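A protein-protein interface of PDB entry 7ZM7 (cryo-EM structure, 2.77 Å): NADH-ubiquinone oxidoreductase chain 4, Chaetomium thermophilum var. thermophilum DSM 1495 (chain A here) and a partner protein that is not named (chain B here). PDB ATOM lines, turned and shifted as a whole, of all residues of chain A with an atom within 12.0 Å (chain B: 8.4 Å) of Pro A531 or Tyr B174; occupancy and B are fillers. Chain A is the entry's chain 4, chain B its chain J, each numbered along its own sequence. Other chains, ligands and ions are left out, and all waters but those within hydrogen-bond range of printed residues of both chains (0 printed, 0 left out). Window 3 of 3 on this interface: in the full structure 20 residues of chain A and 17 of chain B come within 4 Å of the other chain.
The backbone carbonyl oxygen of Gly B167 lies within hydrogen-bond range of the backbone NH of Ile A529, 3.4 Å away. The backbone carbonyl oxygen (O) of Ile A529 lies within hydrogen-bond range of the backbone NH (N) of Lys B169 (2.8 Å). The side-chain amino group (NZ) of Lys B169 lies within salt-bridge range of the side-chain carboxylate (OE1) of Glu A530. The side-chain carboxylate (OE2) of Glu A530 sits close to the backbone carbonyl oxygen (O) of Gly B167, at 3.5 Å. The backbone carbonyl oxygen (O) of Lys B169 sits close to the backbone nitrogen (N) of Pro A531, 3.2 Å away.
NZ of Lys B169 sits at hydrogen-bond distance from OH of Tyr B174, at 3.0 Å. NH2 of Arg B176 lies within hydrogen-bond range of O of Pro B171. The side-chain hydroxyl (OG) of Ser A534 lies within hydrogen-bond range of the backbone carbonyl oxygen (O) of Glu A530.
Ile B168 touches Tyr A527. Gly A528 touches Gly B167. CA of Gly A528 touches CD1 of Ile B168, at 3.7 Å. Ile A529 touches Ile B168. Pro B170 touches Ile A529. Pro B170 touches Pro A531. O of Pro A531 touches CA of Pro B171, at 3.8 Å. Tyr B174 touches Pro A531 (CE2 to CG, 3.6 Å).
Of the printed residues of chain B, Tyr A527 touches Ile B168. Printed residues of chain B within 4 Å of Gly A528: Gly B167 and Ile B168. Pro A531 touches just these residues of chain B: Lys B169 (3.2 Å), Pro B170 (3.6 Å), Pro B171 (3.8 Å) and Tyr B174 (3.6 Å). Tyr A535 touches none of the printed residues of chain B. Of the printed residues of chain A, Ile B168 touches Tyr A527, Gly A528 and Ile A529. Lys B169 touches just these residues of chain A: Ile A529 (2.8 Å), Glu A530 (3.3 Å) and Pro A531 (3.2 Å). Printed residues of chain A within 4 Å of Pro B170: Ile A529 (3.6 Å) and Pro A531 (3.6 Å). No residue of chain A comes within 4 Å of Tyr B173. Of the printed residues of chain A, Tyr B174 touches Pro A531. No residue of chain A comes within 4 Å of Glu B175. No residue of chain A comes within 4 Å of Arg B176. No residue of chain A comes within 4 Å of Ala B178. The nearest residue of chain B that does not touch Pro A531 is Gly B172 (4.02 Å). The nearest printed residue of chain B that does not touch Glu A530 is Tyr B174 (5.0 Å).
Of the 16 printed residues of chain B, 6 touch a printed residue of chain A. Hydrophobic or aromatic side chains of chain B within 4 Å of the printed part of chain A: Ile B168, Pro B171 and Tyr B174. Among the printed residues, Asp or Glu carboxylates within 4 Å of a Lys or Arg side-chain nitrogen of the other chain: Glu A530 with Lys B169 (3.3 Å).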
ATOM      1  N   GLU A 445       3.665  -0.871   4.397  1.00  0.00           N
ATOM      2  CA  GLU A 445       4.488  -1.568   3.371  1.00  0.00           C
ATOM      3  C   GLU A 445       3.951  -2.990   3.178  1.00  0.00           C
ATOM      4  O   GLU A 445       3.977  -3.478   2.035  1.00  0.00           O
ATOM      5  CB  GLU A 445       5.967  -1.545   3.761  1.00  0.00           C
ATOM      6  CG  GLU A 445       6.861  -2.273   2.776  1.00  0.00           C
ATOM      7  CD  GLU A 445       8.353  -2.115   3.005  1.00  0.00           C
ATOM      8  OE1 GLU A 445       8.750  -1.849   4.154  1.00  0.00           O
ATOM      9  OE2 GLU A 445       9.114  -2.248   2.029  1.00  0.00           O
ATOM     10  N   TYR A 527      10.723 -13.026   7.925  1.00  0.00           N
ATOM     11  CA  TYR A 527      10.518 -14.143   7.013  1.00  0.00           C
ATOM     12  C   TYR A 527      10.532 -13.622   5.585  1.00  0.00           C
ATOM     13  O   TYR A 527       9.632 -12.880   5.192  1.00  0.00           O
ATOM     14  CB  TYR A 527       9.193 -14.828   7.322  1.00  0.00           C
ATOM     15  CG  TYR A 527       8.937 -16.136   6.631  1.00  0.00           C
ATOM     16  CD1 TYR A 527       9.748 -17.224   6.853  1.00  0.00           C
ATOM     17  CD2 TYR A 527       7.850 -16.291   5.787  1.00  0.00           C
ATOM     18  CE1 TYR A 527       9.499 -18.420   6.242  1.00  0.00           C
ATOM     19  CE2 TYR A 527       7.592 -17.478   5.179  1.00  0.00           C
ATOM     20  CZ  TYR A 527       8.423 -18.545   5.402  1.00  0.00           C
ATOM     21  OH  TYR A 527       8.178 -19.750   4.792  1.00  0.00           O
ATOM     22  N   GLY A 528      11.536 -14.001   4.813  1.00  0.00           N
ATOM     23  CA  GLY A 528      11.524 -13.686   3.400  1.00  0.00           C
ATOM     24  C   GLY A 528      12.883 -13.818   2.758  1.00  0.00           C
ATOM     25  O   GLY A 528      13.900 -13.984   3.413  1.00  0.00           O
ATOM     26  N   ILE A 529      12.873 -13.730   1.433  1.00  0.00           N
ATOM     27  CA  ILE A 529      14.081 -13.734   0.621  1.00  0.00           C
ATOM     28  C   ILE A 529      13.900 -12.750  -0.516  1.00  0.00           C
ATOM     29  O   ILE A 529      12.779 -12.452  -0.926  1.00  0.00           O
ATOM     30  CB  ILE A 529      14.426 -15.141   0.065  1.00  0.00           C
ATOM     31  CG1 ILE A 529      13.314 -15.661  -0.834  1.00  0.00           C
ATOM     32  CG2 ILE A 529      14.776 -16.109   1.143  1.00  0.00           C
ATOM     33  CD1 ILE A 529      13.698 -16.885  -1.560  1.00  0.00           C
ATOM     34  N   GLU A 530      15.018 -12.242  -1.014  1.00  0.00           N
ATOM     35  CA  GLU A 530      15.130 -11.429  -2.210  1.00  0.00           C
ATOM     36  C   GLU A 530      15.913 -12.192  -3.268  1.00  0.00           C
ATOM     37  O   GLU A 530      16.800 -12.984  -2.936  1.00  0.00           O
ATOM     38  CB  GLU A 530      15.819 -10.095  -1.891  1.00  0.00           C
ATOM     39  CG  GLU A 530      15.134  -9.235  -0.843  1.00  0.00           C
ATOM     40  CD  GLU A 530      13.633  -9.113  -1.054  1.00  0.00           C
ATOM     41  OE1 GLU A 530      13.233  -8.351  -1.956  1.00  0.00           O
ATOM     42  OE2 GLU A 530      12.849  -9.749  -0.326  1.00  0.00           O
ATOM     43  N   PRO A 531      15.624 -11.981  -4.555  1.00  0.00           N
ATOM     44  CA  PRO A 531      16.065 -12.959  -5.561  1.00  0.00           C
ATOM     45  C   PRO A 531      17.561 -13.011  -5.772  1.00  0.00           C
ATOM     46  O   PRO A 531      18.092 -14.095  -6.030  1.00  0.00           O
ATOM     47  CB  PRO A 531      15.344 -12.516  -6.833  1.00  0.00           C
ATOM     48  CG  PRO A 531      14.774 -11.185  -6.545  1.00  0.00           C
ATOM     49  CD  PRO A 531      15.096 -10.759  -5.168  1.00  0.00           C
ATOM     50  N   ASN A 532      18.259 -11.888  -5.652  1.00  0.00           N
ATOM     51  CA  ASN A 532      19.708 -11.908  -5.969  1.00  0.00           C
ATOM     52  C   ASN A 532      20.524 -11.980  -4.680  1.00  0.00           C
ATOM     53  O   ASN A 532      21.750 -12.134  -4.768  1.00  0.00           O
ATOM     54  CB  ASN A 532      20.069 -10.757  -6.906  1.00  0.00           C
ATOM     55  CG  ASN A 532      19.423 -10.896  -8.268  1.00  0.00           C
ATOM     56  OD1 ASN A 532      18.265 -10.533  -8.454  1.00  0.00           O
ATOM     57  ND2 ASN A 532      20.163 -11.431  -9.225  1.00  0.00           N
ATOM     58  N   ALA A 533      19.858 -11.892  -3.529  1.00  0.00           N
ATOM     59  CA  ALA A 533      20.556 -11.929  -2.227  1.00  0.00           C
ATOM     60  C   ALA A 533      20.414 -13.287  -1.545  1.00  0.00           C
ATOM     61  O   ALA A 533      21.057 -13.476  -0.506  1.00  0.00           O
ATOM     62  CB  ALA A 533      19.958 -10.864  -1.345  1.00  0.00           C
ATOM     63  N   SER A 534      19.584 -14.185  -2.068  1.00  0.00           N
ATOM     64  CA  SER A 534      19.366 -15.438  -1.310  1.00  0.00           C
ATOM     65  C   SER A 534      20.095 -16.636  -1.902  1.00  0.00           C
ATOM     66  O   SER A 534      20.545 -16.536  -3.056  1.00  0.00           O
ATOM     67  CB  SER A 534      17.898 -15.727  -1.188  1.00  0.00           C
ATOM     68  OG  SER A 534      17.225 -15.516  -2.419  1.00  0.00           O
ATOM     69  N   TYR A 535      20.255 -17.697  -1.116  1.00  0.00           N
ATOM     70  CA  TYR A 535      20.802 -18.959  -1.616  1.00  0.00           C
ATOM     71  C   TYR A 535      22.149 -18.748  -2.305  1.00  0.00           C
ATOM     72  O   TYR A 535      22.337 -19.047  -3.484  1.00  0.00           O
ATOM     73  CB  TYR A 535      19.801 -19.651  -2.535  1.00  0.00           C
ATOM     74  CG  TYR A 535      18.607 -20.164  -1.792  1.00  0.00           C
ATOM     75  CD1 TYR A 535      18.725 -21.222  -0.925  1.00  0.00           C
ATOM     76  CD2 TYR A 535      17.368 -19.572  -1.935  1.00  0.00           C
ATOM     77  CE1 TYR A 535      17.652 -21.680  -0.230  1.00  0.00           C
ATOM     78  CE2 TYR A 535      16.298 -20.022  -1.237  1.00  0.00           C
ATOM     79  CZ  TYR A 535      16.445 -21.080  -0.387  1.00  0.00           C
ATOM     80  OH  TYR A 535      15.378 -21.567   0.314  1.00  0.00           O
ATOM     81  N   LEU A 536      23.095 -18.230  -1.533  1.00  0.00           N
ATOM     82  CA  LEU A 536      24.377 -17.830  -2.087  1.00  0.00           C
ATOM     83  C   LEU A 536      25.284 -19.038  -2.282  1.00  0.00           C
ATOM     84  O   LEU A 536      25.129 -20.075  -1.634  1.00  0.00           O
ATOM     85  CB  LEU A 536      25.047 -16.817  -1.168  1.00  0.00           C
ATOM     86  CG  LEU A 536      24.202 -15.594  -0.824  1.00  0.00           C
ATOM     87  CD1 LEU A 536      25.075 -14.523  -0.193  1.00  0.00           C
ATOM     88  CD2 LEU A 536      23.488 -15.058  -2.050  1.00  0.00           C
ATOM     89  N   THR A 537      26.246 -18.894  -3.186  1.00  0.00           N
ATOM     90  CA  THR A 537      27.207 -19.959  -3.446  1.00  0.00           C
ATOM     91  C   THR A 537      28.636 -19.466  -3.261  1.00  0.00           C
ATOM     92  O   THR A 537      29.509 -20.213  -2.823  1.00  0.00           O
ATOM     93  CB  THR A 537      27.051 -20.522  -4.864  1.00  0.00           C
ATOM     94  OG1 THR A 537      27.172 -19.460  -5.816  1.00  0.00           O
ATOM     95  CG2 THR A 537      25.694 -21.184  -5.024  1.00  0.00           C
ATOM     96  N   GLY B 167       7.084 -10.119  -0.201  1.00  0.00           N
ATOM     97  CA  GLY B 167       8.427 -10.177   0.404  1.00  0.00           C
ATOM     98  C   GLY B 167       9.064 -11.531   0.234  1.00  0.00           C
ATOM     99  O   GLY B 167      10.193 -11.710   0.707  1.00  0.00           O
ATOM    100  N   ILE B 168       8.333 -12.472  -0.347  1.00  0.00           N
ATOM    101  CA  ILE B 168       8.959 -13.772  -0.680  1.00  0.00           C
ATOM    102  C   ILE B 168       9.298 -13.656  -2.159  1.00  0.00           C
ATOM    103  O   ILE B 168       8.432 -13.958  -2.978  1.00  0.00           O
ATOM    104  CB  ILE B 168       8.003 -14.940  -0.385  1.00  0.00           C
ATOM    105  CG1 ILE B 168       7.382 -14.832   1.009  1.00  0.00           C
ATOM    106  CG2 ILE B 168       8.700 -16.277  -0.595  1.00  0.00           C
ATOM    107  CD1 ILE B 168       8.351 -15.088   2.134  1.00  0.00           C
ATOM    108  N   LYS B 169      10.515 -13.212  -2.468  1.00  0.00           N
ATOM    109  CA  LYS B 169      10.928 -13.036  -3.884  1.00  0.00           C
ATOM    110  C   LYS B 169      11.969 -14.110  -4.180  1.00  0.00           C
ATOM    111  O   LYS B 169      13.163 -13.868  -3.975  1.00  0.00           O
ATOM    112  CB  LYS B 169      11.331 -11.578  -4.120  1.00  0.00           C
ATOM    113  CG  LYS B 169      10.177 -10.596  -3.956  1.00  0.00           C
ATOM    114  CD  LYS B 169      10.597  -9.170  -3.712  1.00  0.00           C
ATOM    115  CE  LYS B 169      11.277  -8.533  -4.901  1.00  0.00           C
ATOM    116  NZ  LYS B 169      11.688  -7.140  -4.610  1.00  0.00           N
ATOM    117  N   PRO B 170      11.550 -15.292  -4.672  1.00  0.00           N
ATOM    118  CA  PRO B 170      12.465 -16.413  -4.879  1.00  0.00           C
ATOM    119  C   PRO B 170      13.360 -16.115  -6.081  1.00  0.00           C
ATOM    120  O   PRO B 170      13.007 -15.267  -6.861  1.00  0.00           O
ATOM    121  CB  PRO B 170      11.532 -17.619  -5.074  1.00  0.00           C
ATOM    122  CG  PRO B 170      10.178 -17.116  -4.639  1.00  0.00           C
ATOM    123  CD  PRO B 170      10.180 -15.651  -5.013  1.00  0.00           C
ATOM    124  N   PRO B 171      14.521 -16.772  -6.237  1.00  0.00           N
ATOM    125  CA  PRO B 171      15.420 -16.409  -7.328  1.00  0.00           C
ATOM    126  C   PRO B 171      14.662 -16.513  -8.653  1.00  0.00           C
ATOM    127  O   PRO B 171      14.049 -17.526  -8.891  1.00  0.00           O
ATOM    128  CB  PRO B 171      16.515 -17.469  -7.203  1.00  0.00           C
ATOM    129  CG  PRO B 171      16.494 -17.867  -5.745  1.00  0.00           C
ATOM    130  CD  PRO B 171      15.027 -17.842  -5.378  1.00  0.00           C
ATOM    131  N   GLY B 172      14.743 -15.477  -9.490  1.00  0.00           N
ATOM    132  CA  GLY B 172      13.980 -15.452 -10.755  1.00  0.00           C
ATOM    133  C   GLY B 172      12.614 -14.774 -10.682  1.00  0.00           C
ATOM    134  O   GLY B 172      11.891 -14.845 -11.689  1.00  0.00           O
ATOM    135  N   TYR B 173      12.259 -14.135  -9.563  1.00  0.00           N
ATOM    136  CA  TYR B 173      10.921 -13.499  -9.403  1.00  0.00           C
ATOM    137  C   TYR B 173      10.740 -12.379 -10.428  1.00  0.00           C
ATOM    138  O   TYR B 173       9.623 -12.237 -10.944  1.00  0.00           O
ATOM    139  CB  TYR B 173      10.739 -12.946  -7.986  1.00  0.00           C
ATOM    140  CG  TYR B 173       9.497 -12.134  -7.721  1.00  0.00           C
ATOM    141  CD1 TYR B 173       8.287 -12.744  -7.441  1.00  0.00           C
ATOM    142  CD2 TYR B 173       9.540 -10.750  -7.711  1.00  0.00           C
ATOM    143  CE1 TYR B 173       7.148 -12.001  -7.186  1.00  0.00           C
ATOM    144  CE2 TYR B 173       8.410  -9.992  -7.460  1.00  0.00           C
ATOM    145  CZ  TYR B 173       7.208 -10.621  -7.199  1.00  0.00           C
ATOM    146  OH  TYR B 173       6.091  -9.882  -6.946  1.00  0.00           O
ATOM    147  N   TYR B 174      11.783 -11.592 -10.688  1.00  0.00           N
ATOM    148  CA  TYR B 174      11.667 -10.431 -11.609  1.00  0.00           C
ATOM    149  C   TYR B 174      11.341 -10.872 -13.043  1.00  0.00           C
ATOM    150  O   TYR B 174      10.448 -10.272 -13.667  1.00  0.00           O
ATOM    151  CB  TYR B 174      12.965  -9.620 -11.571  1.00  0.00           C
ATOM    152  CG  TYR B 174      13.197  -8.889 -10.274  1.00  0.00           C
ATOM    153  CD1 TYR B 174      12.168  -8.210  -9.645  1.00  0.00           C
ATOM    154  CD2 TYR B 174      14.445  -8.868  -9.677  1.00  0.00           C
ATOM    155  CE1 TYR B 174      12.368  -7.534  -8.454  1.00  0.00           C
ATOM    156  CE2 TYR B 174      14.665  -8.193  -8.489  1.00  0.00           C
ATOM    157  CZ  TYR B 174      13.623  -7.525  -7.873  1.00  0.00           C
ATOM    158  OH  TYR B 174      13.836  -6.861  -6.699  1.00  0.00           O
ATOM    159  N   GLU B 175      12.043 -11.886 -13.545  1.00  0.00           N
ATOM    160  CA  GLU B 175      11.814 -12.372 -14.929  1.00  0.00           C
ATOM    161  C   GLU B 175      10.408 -12.964 -15.021  1.00  0.00           C
ATOM    162  O   GLU B 175       9.750 -12.773 -16.051  1.00  0.00           O
ATOM    163  CB  GLU B 175      12.885 -13.393 -15.316  1.00  0.00           C
ATOM    164  N   ARG B 176       9.998 -13.702 -13.998  1.00  0.00           N
ATOM    165  CA  ARG B 176       8.617 -14.234 -13.984  1.00  0.00           C
ATOM    166  C   ARG B 176       7.639 -13.058 -13.913  1.00  0.00           C
ATOM    167  O   ARG B 176       6.630 -13.091 -14.627  1.00  0.00           O
ATOM    168  CB  ARG B 176       8.432 -15.241 -12.847  1.00  0.00           C
ATOM    169  CG  ARG B 176       9.270 -16.502 -12.976  1.00  0.00           C
ATOM    170  CD  ARG B 176       8.859 -17.556 -11.964  1.00  0.00           C
ATOM    171  NE  ARG B 176       8.669 -17.007 -10.628  1.00  0.00           N
ATOM    172  CZ  ARG B 176       9.601 -16.969  -9.680  1.00  0.00           C
ATOM    173  NH1 ARG B 176       9.320 -16.442  -8.502  1.00  0.00           N
ATOM    174  NH2 ARG B 176      10.804 -17.461  -9.911  1.00  0.00           N
ATOM    175  N   ARG B 177       7.941 -12.055 -13.087  1.00  0.00           N
ATOM    176  CA  ARG B 177       7.001 -10.924 -12.899  1.00  0.00           C
ATOM    177  C   ARG B 177       6.888 -10.232 -14.238  1.00  0.00           C
ATOM    178  O   ARG B 177       5.772  -9.811 -14.590  1.00  0.00           O
ATOM    179  CB  ARG B 177       7.480  -9.963 -11.805  1.00  0.00           C
ATOM    180  CG  ARG B 177       6.472  -8.890 -11.419  1.00  0.00           C
ATOM    181  CD  ARG B 177       7.028  -7.945 -10.373  1.00  0.00           C
ATOM    182  NE  ARG B 177       7.488  -6.708 -10.983  1.00  0.00           N
ATOM    183  CZ  ARG B 177       6.873  -5.540 -10.868  1.00  0.00           C
ATOM    184  NH1 ARG B 177       7.360  -4.474 -11.470  1.00  0.00           N
ATOM    185  NH2 ARG B 177       5.780  -5.434 -10.138  1.00  0.00           N
ATOM    186  N   ALA B 178       8.011 -10.118 -14.943  1.00  0.00           N
ATOM    187  CA  ALA B 178       7.936  -9.553 -16.283  1.00  0.00           C
ATOM    188  C   ALA B 178       6.878 -10.270 -17.100  1.00  0.00           C
ATOM    189  O   ALA B 178       5.999  -9.639 -17.692  1.00  0.00           O
ATOM    190  CB  ALA B 178       9.297  -9.647 -16.967  1.00  0.00           C
ATOM    191  N   GLN B 179       6.917 -11.600 -17.093  1.00  0.00           N
ATOM    192  CA  GLN B 179       5.943 -12.371 -17.848  1.00  0.00           C
ATOM    193  C   GLN B 179       4.529 -12.153 -17.328  1.00  0.00           C
ATOM    194  O   GLN B 179       3.595 -11.958 -18.109  1.00  0.00           O
ATOM    195  CB  GLN B 179       6.310 -13.852 -17.798  1.00  0.00           C
ATOM    196  CG  GLN B 179       5.389 -14.717 -18.624  1.00  0.00           C
ATOM    197  CD  GLN B 179       5.522 -14.421 -20.098  1.00  0.00           C
ATOM    198  OE1 GLN B 179       6.626 -14.227 -20.605  1.00  0.00           O
ATOM    199  NE2 GLN B 179       4.394 -14.366 -20.793  1.00  0.00           N
ATOM    200  N   ARG B 180       4.352 -12.184 -16.014  1.00  0.00           N
ATOM    201  CA  ARG B 180       3.016 -12.056 -15.452  1.00  0.00           C
ATOM    202  C   ARG B 180       2.391 -10.718 -15.825  1.00  0.00           C
ATOM    203  O   ARG B 180       1.213 -10.652 -16.192  1.00  0.00           O
ATOM    204  CB  ARG B 180       3.089 -12.217 -13.943  1.00  0.00           C
ATOM    205  CG  ARG B 180       1.772 -12.441 -13.257  1.00  0.00           C
ATOM    206  CD  ARG B 180       2.001 -12.943 -11.839  1.00  0.00           C
ATOM    207  NE  ARG B 180       2.605 -11.927 -10.980  1.00  0.00           N
ATOM    208  CZ  ARG B 180       3.901 -11.864 -10.691  1.00  0.00           C
ATOM    209  NH1 ARG B 180       4.356 -10.908  -9.900  1.00  0.00           N
ATOM    210  NH2 ARG B 180       4.745 -12.745 -11.204  1.00  0.00           N
ATOM    211  N   LEU B 181       3.172  -9.641 -15.744  1.00  0.00           N
ATOM    212  CA  LEU B 181       2.653  -8.328 -16.089  1.00  0.00           C
ATOM    213  C   LEU B 181       2.378  -8.218 -17.577  1.00  0.00           C
ATOM    214  O   LEU B 181       1.384  -7.607 -17.983  1.00  0.00           O
ATOM    215  CB  LEU B 181       3.632  -7.248 -15.640  1.00  0.00           C
ATOM    216  CG  LEU B 181       3.594  -6.928 -14.149  1.00  0.00           C
ATOM    217  CD1 LEU B 181       4.530  -5.786 -13.820  1.00  0.00           C
ATOM    218  CD2 LEU B 181       2.174  -6.597 -13.732  1.00  0.00           C
ATOM    219  N   ILE B 189       8.076  -4.320 -19.915  1.00  0.00           N
ATOM    220  CA  ILE B 189       8.806  -3.679 -18.829  1.00  0.00           C
ATOM    221  C   ILE B 189      10.189  -3.275 -19.312  1.00  0.00           C
ATOM    222  O   ILE B 189      10.938  -4.095 -19.854  1.00  0.00           O
ATOM    223  CB  ILE B 189       8.903  -4.605 -17.611  1.00  0.00           C
ATOM    224  CG1 ILE B 189       7.534  -4.756 -16.954  1.00  0.00           C
ATOM    225  CG2 ILE B 189       9.943  -4.088 -16.635  1.00  0.00           C
ATOM    226  CD1 ILE B 189       7.571  -5.522 -15.670  1.00  0.00           C
